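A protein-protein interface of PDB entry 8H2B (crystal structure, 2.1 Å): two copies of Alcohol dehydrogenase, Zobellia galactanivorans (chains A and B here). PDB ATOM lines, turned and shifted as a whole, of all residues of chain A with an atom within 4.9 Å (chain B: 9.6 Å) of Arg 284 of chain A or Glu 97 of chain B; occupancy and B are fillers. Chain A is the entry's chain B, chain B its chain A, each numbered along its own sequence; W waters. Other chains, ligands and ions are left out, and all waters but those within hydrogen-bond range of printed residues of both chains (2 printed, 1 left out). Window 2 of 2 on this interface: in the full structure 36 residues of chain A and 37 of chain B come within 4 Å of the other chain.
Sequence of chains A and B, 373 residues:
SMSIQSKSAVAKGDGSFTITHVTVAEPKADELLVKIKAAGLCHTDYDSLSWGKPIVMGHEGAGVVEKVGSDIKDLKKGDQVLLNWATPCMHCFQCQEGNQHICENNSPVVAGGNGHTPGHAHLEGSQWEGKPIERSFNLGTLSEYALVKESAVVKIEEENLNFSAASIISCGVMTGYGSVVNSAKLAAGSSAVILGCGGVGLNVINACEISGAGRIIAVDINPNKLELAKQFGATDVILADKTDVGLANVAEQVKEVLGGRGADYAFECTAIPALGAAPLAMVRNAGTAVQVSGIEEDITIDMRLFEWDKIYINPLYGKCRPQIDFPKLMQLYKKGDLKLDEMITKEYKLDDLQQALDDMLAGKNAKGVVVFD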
ATOM      1  N   ARG A 261       7.738 -23.767 -35.309  1.00  0.00           N
ATOM      2  CA  ARG A 261       7.180 -24.628 -34.274  1.00  0.00           C
ATOM      3  C   ARG A 261       5.669 -24.646 -34.436  1.00  0.00           C
ATOM      4  O   ARG A 261       5.076 -23.674 -34.923  1.00  0.00           O
ATOM      5  CB  ARG A 261       7.593 -24.146 -32.863  1.00  0.00           C
ATOM      6  CG  ARG A 261       7.162 -25.074 -31.731  1.00  0.00           C
ATOM      7  CD  ARG A 261       7.644 -24.613 -30.357  1.00  0.00           C
ATOM      8  NE  ARG A 261       9.102 -24.575 -30.237  1.00  0.00           N
ATOM      9  CZ  ARG A 261       9.805 -23.453 -30.114  1.00  0.00           C
ATOM     10  NH1 ARG A 261       9.176 -22.286 -30.089  1.00  0.00           N
ATOM     11  NH2 ARG A 261      11.133 -23.491 -30.017  1.00  0.00           N
ATOM     12  N   GLY A 262       5.052 -25.766 -34.071  1.00  0.00           N
ATOM     13  CA  GLY A 262       3.603 -25.872 -34.132  1.00  0.00           C
ATOM     14  C   GLY A 262       2.908 -24.930 -33.156  1.00  0.00           C
ATOM     15  O   GLY A 262       3.515 -24.345 -32.255  1.00  0.00           O
ATOM     16  N   ALA A 263       1.587 -24.812 -33.332  1.00  0.00           N
ATOM     17  CA  ALA A 263       0.762 -23.948 -32.490  1.00  0.00           C
ATOM     18  C   ALA A 263       0.623 -24.499 -31.070  1.00  0.00           C
ATOM     19  O   ALA A 263       0.837 -25.687 -30.806  1.00  0.00           O
ATOM     20  CB  ALA A 263      -0.634 -23.792 -33.096  1.00  0.00           C
ATOM     21  N   ASP A 264       0.239 -23.610 -30.144  1.00  0.00           N
ATOM     22  CA  ASP A 264      -0.094 -24.048 -28.792  1.00  0.00           C
ATOM     23  C   ASP A 264      -1.435 -24.780 -28.756  1.00  0.00           C
ATOM     24  O   ASP A 264      -1.589 -25.764 -28.020  1.00  0.00           O
ATOM     25  CB  ASP A 264      -0.116 -22.862 -27.827  1.00  0.00           C
ATOM     26  CG  ASP A 264       1.217 -22.106 -27.784  1.00  0.00           C
ATOM     27  OD1 ASP A 264       2.279 -22.779 -27.773  1.00  0.00           O
ATOM     28  OD2 ASP A 264       1.205 -20.845 -27.766  1.00  0.00           O
ATOM     29  N   MET A 282      -1.427 -29.859 -36.153  1.00  0.00           N
ATOM     30  CA  MET A 282      -1.225 -28.422 -36.072  1.00  0.00           C
ATOM     31  C   MET A 282      -0.420 -27.986 -34.852  1.00  0.00           C
ATOM     32  O   MET A 282       0.146 -26.886 -34.879  1.00  0.00           O
ATOM     33  CB  MET A 282      -2.584 -27.704 -36.049  1.00  0.00           C
ATOM     34  CG  MET A 282      -3.508 -28.041 -37.192  1.00  0.00           C
ATOM     35  SD  MET A 282      -2.778 -27.739 -38.812  1.00  0.00           S
ATOM     36  CE  MET A 282      -3.535 -29.098 -39.738  1.00  0.00           C
ATOM     37  N   VAL A 283      -0.376 -28.778 -33.771  1.00  0.00           N
ATOM     38  CA  VAL A 283       0.198 -28.284 -32.520  1.00  0.00           C
ATOM     39  C   VAL A 283       1.575 -28.893 -32.271  1.00  0.00           C
ATOM     40  O   VAL A 283       1.903 -29.997 -32.726  1.00  0.00           O
ATOM     41  CB  VAL A 283      -0.723 -28.536 -31.307  1.00  0.00           C
ATOM     42  CG1 VAL A 283      -2.087 -27.888 -31.549  1.00  0.00           C
ATOM     43  CG2 VAL A 283      -0.826 -30.036 -30.987  1.00  0.00           C
ATOM     44  N   ARG A 284       2.392 -28.136 -31.546  1.00  0.00           N
ATOM     45  CA  ARG A 284       3.679 -28.592 -31.050  1.00  0.00           C
ATOM     46  C   ARG A 284       3.484 -29.734 -30.046  1.00  0.00           C
ATOM     47  O   ARG A 284       2.375 -29.999 -29.572  1.00  0.00           O
ATOM     48  CB  ARG A 284       4.398 -27.439 -30.359  1.00  0.00           C
ATOM     49  CG  ARG A 284       3.559 -26.843 -29.209  1.00  0.00           C
ATOM     50  CD  ARG A 284       4.450 -25.961 -28.327  1.00  0.00           C
ATOM     51  NE  ARG A 284       3.747 -25.148 -27.334  1.00  0.00           N
ATOM     52  CZ  ARG A 284       3.436 -25.573 -26.112  1.00  0.00           C
ATOM     53  NH1 ARG A 284       3.723 -26.822 -25.746  1.00  0.00           N
ATOM     54  NH2 ARG A 284       2.829 -24.756 -25.256  1.00  0.00           N
ATOM     55  N   ASN A 285       4.583 -30.389 -29.690  1.00  0.00           N
ATOM     56  CA  ASN A 285       4.530 -31.318 -28.567  1.00  0.00           C
ATOM     57  C   ASN A 285       4.068 -30.566 -27.326  1.00  0.00           C
ATOM     58  O   ASN A 285       4.375 -29.379 -27.156  1.00  0.00           O
ATOM     59  CB  ASN A 285       5.893 -31.968 -28.331  1.00  0.00           C
ATOM     60  CG  ASN A 285       6.248 -32.968 -29.410  1.00  0.00           C
ATOM     61  OD1 ASN A 285       5.371 -33.532 -30.054  1.00  0.00           O
ATOM     62  ND2 ASN A 285       7.532 -33.196 -29.608  1.00  0.00           N
ATOM     63  N   ALA A 286       3.299 -31.255 -26.477  1.00  0.00           N
ATOM     64  CA  ALA A 286       2.674 -30.706 -25.277  1.00  0.00           C
ATOM     65  C   ALA A 286       1.617 -29.648 -25.595  1.00  0.00           C
ATOM     66  O   ALA A 286       1.142 -28.958 -24.672  1.00  0.00           O
ATOM     67  CB  ALA A 286       3.715 -30.143 -24.295  1.00  0.00           C
ATOM     68  N   GLY A 287       1.210 -29.512 -26.864  1.00  0.00           N
ATOM     69  CA  GLY A 287       0.106 -28.648 -27.233  1.00  0.00           C
ATOM     70  C   GLY A 287      -1.258 -29.286 -26.961  1.00  0.00           C
ATOM     71  O   GLY A 287      -1.370 -30.428 -26.505  1.00  0.00           O
ATOM     72  N   LYS A 310       0.662 -34.321 -26.282  1.00  0.00           N
ATOM     73  CA  LYS A 310      -0.453 -33.506 -26.739  1.00  0.00           C
ATOM     74  C   LYS A 310      -1.734 -33.929 -26.031  1.00  0.00           C
ATOM     75  O   LYS A 310      -2.034 -35.122 -25.917  1.00  0.00           O
ATOM     76  CB  LYS A 310      -0.612 -33.636 -28.250  1.00  0.00           C
ATOM     77  CG  LYS A 310       0.647 -33.270 -29.032  1.00  0.00           C
ATOM     78  CD  LYS A 310       0.465 -33.591 -30.532  1.00  0.00           C
ATOM     79  CE  LYS A 310       1.756 -33.282 -31.324  1.00  0.00           C
ATOM     80  NZ  LYS A 310       1.498 -33.449 -32.789  1.00  0.00           N
ATOM     81  N   MET B  90      18.225 -27.618 -20.977  1.00  0.00           N
ATOM     82  CA  MET B  90      17.885 -26.671 -19.900  1.00  0.00           C
ATOM     83  C   MET B  90      17.627 -25.272 -20.460  1.00  0.00           C
ATOM     84  O   MET B  90      17.272 -24.369 -19.676  1.00  0.00           O
ATOM     85  CB  MET B  90      18.962 -26.628 -18.797  1.00  0.00           C
ATOM     86  CG  MET B  90      19.114 -27.993 -18.111  1.00  0.00           C
ATOM     87  SD  MET B  90      17.643 -28.417 -17.204  1.00  0.00           S
ATOM     88  CE  MET B  90      16.757 -29.380 -18.311  1.00  0.00           C
ATOM     89  N   HIS B  91      17.736 -25.065 -21.786  1.00  0.00           N
ATOM     90  CA  HIS B  91      17.558 -23.739 -22.384  1.00  0.00           C
ATOM     91  C   HIS B  91      16.533 -23.664 -23.509  1.00  0.00           C
ATOM     92  O   HIS B  91      16.079 -22.553 -23.813  1.00  0.00           O
ATOM     93  CB  HIS B  91      18.903 -23.210 -22.907  1.00  0.00           C
ATOM     94  CG  HIS B  91      19.787 -22.699 -21.816  1.00  0.00           C
ATOM     95  ND1 HIS B  91      20.593 -23.527 -21.061  1.00  0.00           N
ATOM     96  CD2 HIS B  91      19.966 -21.449 -21.325  1.00  0.00           C
ATOM     97  CE1 HIS B  91      21.242 -22.806 -20.162  1.00  0.00           C
ATOM     98  NE2 HIS B  91      20.882 -21.542 -20.303  1.00  0.00           N
ATOM     99  N   CYS B  92      16.144 -24.781 -24.127  1.00  0.00           N
ATOM    100  CA  CYS B  92      15.221 -24.710 -25.248  1.00  0.00           C
ATOM    101  C   CYS B  92      13.813 -24.398 -24.744  1.00  0.00           C
ATOM    102  O   CYS B  92      13.555 -24.359 -23.543  1.00  0.00           O
ATOM    103  CB  CYS B  92      15.235 -26.021 -26.041  1.00  0.00           C
ATOM    104  SG  CYS B  92      14.361 -27.392 -25.189  1.00  0.00           S
ATOM    105  N   PHE B  93      12.902 -24.156 -25.684  1.00  0.00           N
ATOM    106  CA  PHE B  93      11.522 -23.828 -25.338  1.00  0.00           C
ATOM    107  C   PHE B  93      10.895 -24.884 -24.430  1.00  0.00           C
ATOM    108  O   PHE B  93      10.294 -24.562 -23.401  1.00  0.00           O
ATOM    109  CB  PHE B  93      10.690 -23.670 -26.609  1.00  0.00           C
ATOM    110  CG  PHE B  93       9.225 -23.525 -26.342  1.00  0.00           C
ATOM    111  CD1 PHE B  93       8.707 -22.320 -25.896  1.00  0.00           C
ATOM    112  CD2 PHE B  93       8.362 -24.597 -26.514  1.00  0.00           C
ATOM    113  CE1 PHE B  93       7.342 -22.183 -25.623  1.00  0.00           C
ATOM    114  CE2 PHE B  93       7.001 -24.465 -26.245  1.00  0.00           C
ATOM    115  CZ  PHE B  93       6.495 -23.253 -25.802  1.00  0.00           C
ATOM    116  N   GLN B  94      11.021 -26.154 -24.804  1.00  0.00           N
ATOM    117  CA  GLN B  94      10.409 -27.214 -24.014  1.00  0.00           C
ATOM    118  C   GLN B  94      11.042 -27.317 -22.625  1.00  0.00           C
ATOM    119  O   GLN B  94      10.320 -27.426 -21.626  1.00  0.00           O
ATOM    120  CB  GLN B  94      10.477 -28.540 -24.771  1.00  0.00           C
ATOM    121  CG  GLN B  94       9.541 -28.608 -25.992  1.00  0.00           C
ATOM    122  CD  GLN B  94       8.030 -28.531 -25.638  1.00  0.00           C
ATOM    123  OE1 GLN B  94       7.634 -28.420 -24.471  1.00  0.00           O
ATOM    124  NE2 GLN B  94       7.194 -28.567 -26.665  1.00  0.00           N
ATOM    125  N   CYS B  95      12.379 -27.230 -22.526  1.00  0.00           N
ATOM    126  CA  CYS B  95      13.007 -27.225 -21.200  1.00  0.00           C
ATOM    127  C   CYS B  95      12.491 -26.077 -20.337  1.00  0.00           C
ATOM    128  O   CYS B  95      12.283 -26.236 -19.125  1.00  0.00           O
ATOM    129  CB  CYS B  95      14.528 -27.161 -21.328  1.00  0.00           C
ATOM    130  SG  CYS B  95      15.252 -28.754 -21.833  1.00  0.00           S
ATOM    131  N   GLN B  96      12.271 -24.909 -20.937  1.00  0.00           N
ATOM    132  CA  GLN B  96      11.819 -23.782 -20.129  1.00  0.00           C
ATOM    133  C   GLN B  96      10.355 -23.898 -19.739  1.00  0.00           C
ATOM    134  O   GLN B  96       9.927 -23.236 -18.790  1.00  0.00           O
ATOM    135  CB  GLN B  96      12.080 -22.475 -20.872  1.00  0.00           C
ATOM    136  CG  GLN B  96      13.586 -22.202 -20.988  1.00  0.00           C
ATOM    137  CD  GLN B  96      13.892 -20.745 -21.270  1.00  0.00           C
ATOM    138  OE1 GLN B  96      13.310 -19.848 -20.655  1.00  0.00           O
ATOM    139  NE2 GLN B  96      14.818 -20.502 -22.193  1.00  0.00           N
ATOM    140  N   GLU B  97       9.582 -24.703 -20.459  1.00  0.00           N
ATOM    141  CA  GLU B  97       8.212 -25.024 -20.081  1.00  0.00           C
ATOM    142  C   GLU B  97       8.163 -26.050 -18.957  1.00  0.00           C
ATOM    143  O   GLU B  97       7.077 -26.348 -18.439  1.00  0.00           O
ATOM    144  CB  GLU B  97       7.460 -25.554 -21.313  1.00  0.00           C
ATOM    145  CG  GLU B  97       6.906 -24.471 -22.262  1.00  0.00           C
ATOM    146  CD  GLU B  97       5.586 -23.864 -21.764  1.00  0.00           C
ATOM    147  OE1 GLU B  97       5.563 -22.650 -21.459  1.00  0.00           O
ATOM    148  OE2 GLU B  97       4.575 -24.601 -21.677  1.00  0.00           O
ATOM    149  N   GLY B  98       9.312 -26.580 -18.562  1.00  0.00           N
ATOM    150  CA  GLY B  98       9.372 -27.683 -17.638  1.00  0.00           C
ATOM    151  C   GLY B  98       9.313 -29.040 -18.301  1.00  0.00           C
ATOM    152  O   GLY B  98       9.263 -30.058 -17.591  1.00  0.00           O
ATOM    153  N   ASN B  99       9.306 -29.087 -19.630  1.00  0.00           N
ATOM    154  CA  ASN B  99       9.180 -30.341 -20.377  1.00  0.00           C
ATOM    155  C   ASN B  99      10.553 -30.854 -20.798  1.00  0.00           C
ATOM    156  O   ASN B  99      10.888 -30.948 -21.982  1.00  0.00           O
ATOM    157  CB  ASN B  99       8.263 -30.134 -21.575  1.00  0.00           C
ATOM    158  CG  ASN B  99       6.822 -29.870 -21.153  1.00  0.00           C
ATOM    159  OD1 ASN B  99       6.336 -30.441 -20.169  1.00  0.00           O
ATOM    160  ND2 ASN B  99       6.132 -29.026 -21.900  1.00  0.00           N
ATOM    161  N   GLN B 100      11.368 -31.157 -19.785  1.00  0.00           N
ATOM    162  CA  GLN B 100      12.738 -31.616 -20.027  1.00  0.00           C
ATOM    163  C   GLN B 100      12.767 -32.918 -20.817  1.00  0.00           C
ATOM    164  O   GLN B 100      13.745 -33.217 -21.523  1.00  0.00           O
ATOM    165  CB  GLN B 100      13.433 -31.803 -18.680  1.00  0.00           C
ATOM    166  CG  GLN B 100      13.614 -30.492 -17.935  1.00  0.00           C
ATOM    167  CD  GLN B 100      14.366 -30.655 -16.629  1.00  0.00           C
ATOM    168  OE1 GLN B 100      15.093 -31.646 -16.428  1.00  0.00           O
ATOM    169  NE2 GLN B 100      14.236 -29.662 -15.747  1.00  0.00           N
ATOM    170  N   HIS B 101      11.712 -33.704 -20.701  1.00  0.00           N
ATOM    171  CA  HIS B 101      11.614 -35.011 -21.327  1.00  0.00           C
ATOM    172  C   HIS B 101      11.347 -34.927 -22.825  1.00  0.00           C
ATOM    173  O   HIS B 101      11.426 -35.950 -23.512  1.00  0.00           O
ATOM    174  CB  HIS B 101      10.496 -35.767 -20.619  1.00  0.00           C
ATOM    175  CG  HIS B 101       9.177 -35.083 -20.750  1.00  0.00           C
ATOM    176  ND1 HIS B 101       8.899 -33.888 -20.120  1.00  0.00           N
ATOM    177  CD2 HIS B 101       8.078 -35.395 -21.477  1.00  0.00           C
ATOM    178  CE1 HIS B 101       7.682 -33.497 -20.451  1.00  0.00           C
ATOM    179  NE2 HIS B 101       7.157 -34.405 -21.254  1.00  0.00           N
ATOM    180  N   ILE B 102      11.001 -33.753 -23.349  1.00  0.00           N
ATOM    181  CA  ILE B 102      10.906 -33.588 -24.800  1.00  0.00           C
ATOM    182  C   ILE B 102      11.802 -32.432 -25.252  1.00  0.00           C
ATOM    183  O   ILE B 102      11.425 -31.625 -26.111  1.00  0.00           O
ATOM    184  CB  ILE B 102       9.450 -33.378 -25.235  1.00  0.00           C
ATOM    185  CG1 ILE B 102       8.744 -32.413 -24.284  1.00  0.00           C
ATOM    186  CG2 ILE B 102       8.709 -34.716 -25.259  1.00  0.00           C
ATOM    187  CD1 ILE B 102       7.381 -31.929 -24.815  1.00  0.00           C
ATOM    188  N   CYS B 103      12.990 -32.351 -24.665  1.00  0.00           N
ATOM    189  CA  CYS B 103      13.950 -31.312 -24.996  1.00  0.00           C
ATOM    190  C   CYS B 103      14.212 -31.273 -26.502  1.00  0.00           C
ATOM    191  O   CYS B 103      14.533 -32.296 -27.114  1.00  0.00           O
ATOM    192  CB  CYS B 103      15.240 -31.579 -24.224  1.00  0.00           C
ATOM    193  SG  CYS B 103      16.641 -30.600 -24.821  1.00  0.00           S
ATOM    194  N   GLU B 104      14.037 -30.095 -27.107  1.00  0.00           N
ATOM    195  CA  GLU B 104      14.106 -29.994 -28.566  1.00  0.00           C
ATOM    196  C   GLU B 104      15.514 -30.199 -29.110  1.00  0.00           C
ATOM    197  O   GLU B 104      15.663 -30.449 -30.309  1.00  0.00           O
ATOM    198  CB  GLU B 104      13.564 -28.640 -29.042  1.00  0.00           C
ATOM    199  CG  GLU B 104      12.049 -28.485 -28.866  1.00  0.00           C
ATOM    200  CD  GLU B 104      11.554 -27.052 -29.110  1.00  0.00           C
ATOM    201  OE1 GLU B 104      10.322 -26.843 -29.143  1.00  0.00           O
ATOM    202  OE2 GLU B 104      12.391 -26.134 -29.251  1.00  0.00           O
ATOM    203  N   VAL B 110      12.960 -37.229 -29.387  1.00  0.00           N
ATOM    204  CA  VAL B 110      12.355 -36.128 -30.126  1.00  0.00           C
ATOM    205  C   VAL B 110      13.364 -35.380 -30.997  1.00  0.00           C
ATOM    206  O   VAL B 110      12.981 -34.805 -32.022  1.00  0.00           O
ATOM    207  CB  VAL B 110      11.646 -35.191 -29.129  1.00  0.00           C
ATOM    208  CG1 VAL B 110      11.220 -33.916 -29.792  1.00  0.00           C
ATOM    209  CG2 VAL B 110      10.423 -35.905 -28.553  1.00  0.00           C
ATOM    210  N   LYS B 185      -2.038 -36.631 -13.330  1.00  0.00           N
ATOM    211  CA  LYS B 185      -2.228 -35.926 -12.061  1.00  0.00           C
ATOM    212  C   LYS B 185      -3.337 -36.595 -11.242  1.00  0.00           C
ATOM    213  O   LYS B 185      -4.275 -35.956 -10.753  1.00  0.00           O
ATOM    214  CB  LYS B 185      -2.527 -34.448 -12.305  1.00  0.00           C
ATOM    215  CG  LYS B 185      -1.331 -33.677 -12.893  1.00  0.00           C
ATOM    216  CD  LYS B 185      -1.666 -32.187 -13.092  1.00  0.00           C
ATOM    217  CE  LYS B 185      -1.266 -31.700 -14.471  1.00  0.00           C
ATOM    218  NZ  LYS B 185       0.217 -31.550 -14.576  1.00  0.00           N
ATOM    219  N   LYS B 319       6.853 -37.434 -18.216  1.00  0.00           N
ATOM    220  CA  LYS B 319       7.136 -36.002 -18.017  1.00  0.00           C
ATOM    221  C   LYS B 319       8.339 -35.788 -17.103  1.00  0.00           C
ATOM    222  O   LYS B 319       8.385 -34.829 -16.330  1.00  0.00           O
ATOM    223  CB  LYS B 319       5.905 -35.268 -17.478  1.00  0.00           C
ATOM    224  CG  LYS B 319       4.998 -34.801 -18.580  1.00  0.00           C
ATOM    225  CD  LYS B 319       3.624 -34.406 -18.110  1.00  0.00           C
ATOM    226  CE  LYS B 319       2.755 -34.173 -19.332  1.00  0.00           C
ATOM    227  NZ  LYS B 319       2.199 -35.429 -19.942  1.00  0.00           N
ATOM    228  N   ARG B 321      11.435 -34.861 -15.089  1.00  0.00           N
ATOM    229  CA  ARG B 321      12.499 -33.890 -14.847  1.00  0.00           C
ATOM    230  C   ARG B 321      13.510 -34.542 -13.915  1.00  0.00           C
ATOM    231  O   ARG B 321      13.319 -34.536 -12.690  1.00  0.00           O
ATOM    232  CB  ARG B 321      11.956 -32.587 -14.250  1.00  0.00           C
ATOM    233  CG  ARG B 321      11.147 -31.753 -15.243  1.00  0.00           C
ATOM    234  CD  ARG B 321      10.396 -30.635 -14.513  1.00  0.00           C
ATOM    235  NE  ARG B 321       9.550 -31.217 -13.474  1.00  0.00           N
ATOM    236  CZ  ARG B 321       9.101 -30.563 -12.405  1.00  0.00           C
ATOM    237  NH1 ARG B 321       9.399 -29.281 -12.237  1.00  0.00           N
ATOM    238  NH2 ARG B 321       8.356 -31.196 -11.497  1.00  0.00           N
HETATM  239  O   HOH W   1      13.886 -23.463 -28.045  1.00  0.00           O
HETATM  240  O   HOH W   2       9.603 -31.281 -28.413  1.00  0.00           O
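Printed residues of chain B within 4 Å of Arg 261 of chain A: Phe 93 (3.4 Å) and Glu 104 (2.8 Å).
No residue of chain B comes within 4 Å of Gly 262 of chain A.
No residue of chain B comes within 4 Å of Ala 263 of chain A.
No residue of chain B comes within 4 Å of Asp 264 of chain A.
No residue of chain B comes within 4 Å of Val 283 of chain A.
Of the printed residues of chain B, Arg 284 of chain A touches Phe 93 (3.5 Å), Gln 94 (3.99 Å) and Glu 97 (3.99 Å).
Of the printed residues of chain B, Asn 285 of chain A touches Gln 94 (3.0 Å), Ile 102 (3.8 Å) and Val 110 (3.8 Å).
Of chain B, only Asn 99 (3.6 Å) comes within 4 Å of Ala 286 of chain A.
Printed residues of chain A within 4 Å of Phe 93 of chain B: Arg 261 and Arg 284.
Printed residues of chain A within 4 Å of Glu 97 of chain B: Arg 284 (3.99 Å).
Printed residues of chain A within 4 Å of Asn 99 of chain B: Ala 286.
Lys 319 of chain B touches none of the printed residues of chain A.
The nearest printed residue of chain B that does not touch Arg 284 of chain A is Asn 99 of chain B (5.0 Å).
The nearest printed residue of chain A that does not touch Val 110 of chain B is Ala 286 of chain A (8.8 Å).
Hydrophobic or aromatic side chains of chain A within 4 Å of the printed part of chain B: Ala 286.
Along chain A the printed residues that touch a printed residue of chain B span positions 261 to 286.
Printed residues of chain B that touch a printed residue of chain A: Phe 93, Gln 94, Glu 97, Asn 99, Ile 102, Glu 104 and Val 110.
Hydrophobic or aromatic side chains of chain B within 4 Å of the printed part of chain A: Phe 93, Ile 102 and Val 110.
Along chain B the printed residues that touch a printed residue of chain A span positions 93 to 110.
Among the printed residues, 9 pairs touch across the chains.
Among the printed residues, Asp or Glu carboxylates within 4 Å of a Lys or Arg side-chain nitrogen of the other chain: Arg 261 of chain A with Glu 104 of chain B (2.8 Å) and Arg 284 of chain A with Glu 97 of chain B (3.99 Å).
No position is printed for both chains.
Of the 9 pairs that touch across the chains among the printed residues, none has its exchanged pair printed and touching as well.
Water W1 lies within hydrogen-bond range of the backbone NH (N) of Phe 93 of chain B (2.7 Å), the side-chain carboxylate (OE2) of Glu 104 of chain B (3.3 Å) and the guanidinium group (NH2) of Arg 261 of chain A (3.4 Å).
Water W2 lies within hydrogen-bond range of O of Ile 102 of chain B (3.0 Å) and ND2 of Asn 285 of chain A (3.1 Å).
The side-chain sulfur of Cys 92 of chain B lies close to the backbone NH of Gln 94 of chain B (3.6 Å).
The side-chain sulfur (SG) of Cys 92 of chain B sits close to the backbone NH (N) of Glu 104 of chain B (3.3 Å).
O of Gln 94 of chain B lies within hydrogen-bond range of N of Asn 99 of chain B (2.8 Å).
The backbone carbonyl oxygen (O) of Ala 263 of chain A lies within hydrogen-bond range of the backbone NH (N) of Arg 284 of chain A, 3.0 Å away.
The side-chain carboxylate (OD1) of Asp 264 of chain A is in salt-bridge range of the guanidinium group (NE) of Arg 284 of chain A (2.8 Å).
Among the printed residues, pairs that only touch across the chains: Arg 261 of chain A with Phe 93 of chain B, Arg 284 of chain A with Phe 93 of chain B, Ala 286 of chain A with Asn 99 of chain B, Asn 285 of chain A with Val 110 of chain B, Asn 285 of chain A with Ile 102 of chain B and Arg 284 of chain A with Gln 94 of chain B.
NE2 of Gln 94 of chain B is in hydrogen-bond range of O of Asn 285 of chain A (3.0 Å).
OE2 of Glu 97 of chain B is in salt-bridge range of NH2 of Arg 284 of chain A.
The guanidinium group of Arg 261 of chain A is in salt-bridge range of the side-chain carboxylate of Glu 104 of chain B, 2.8 Å away.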
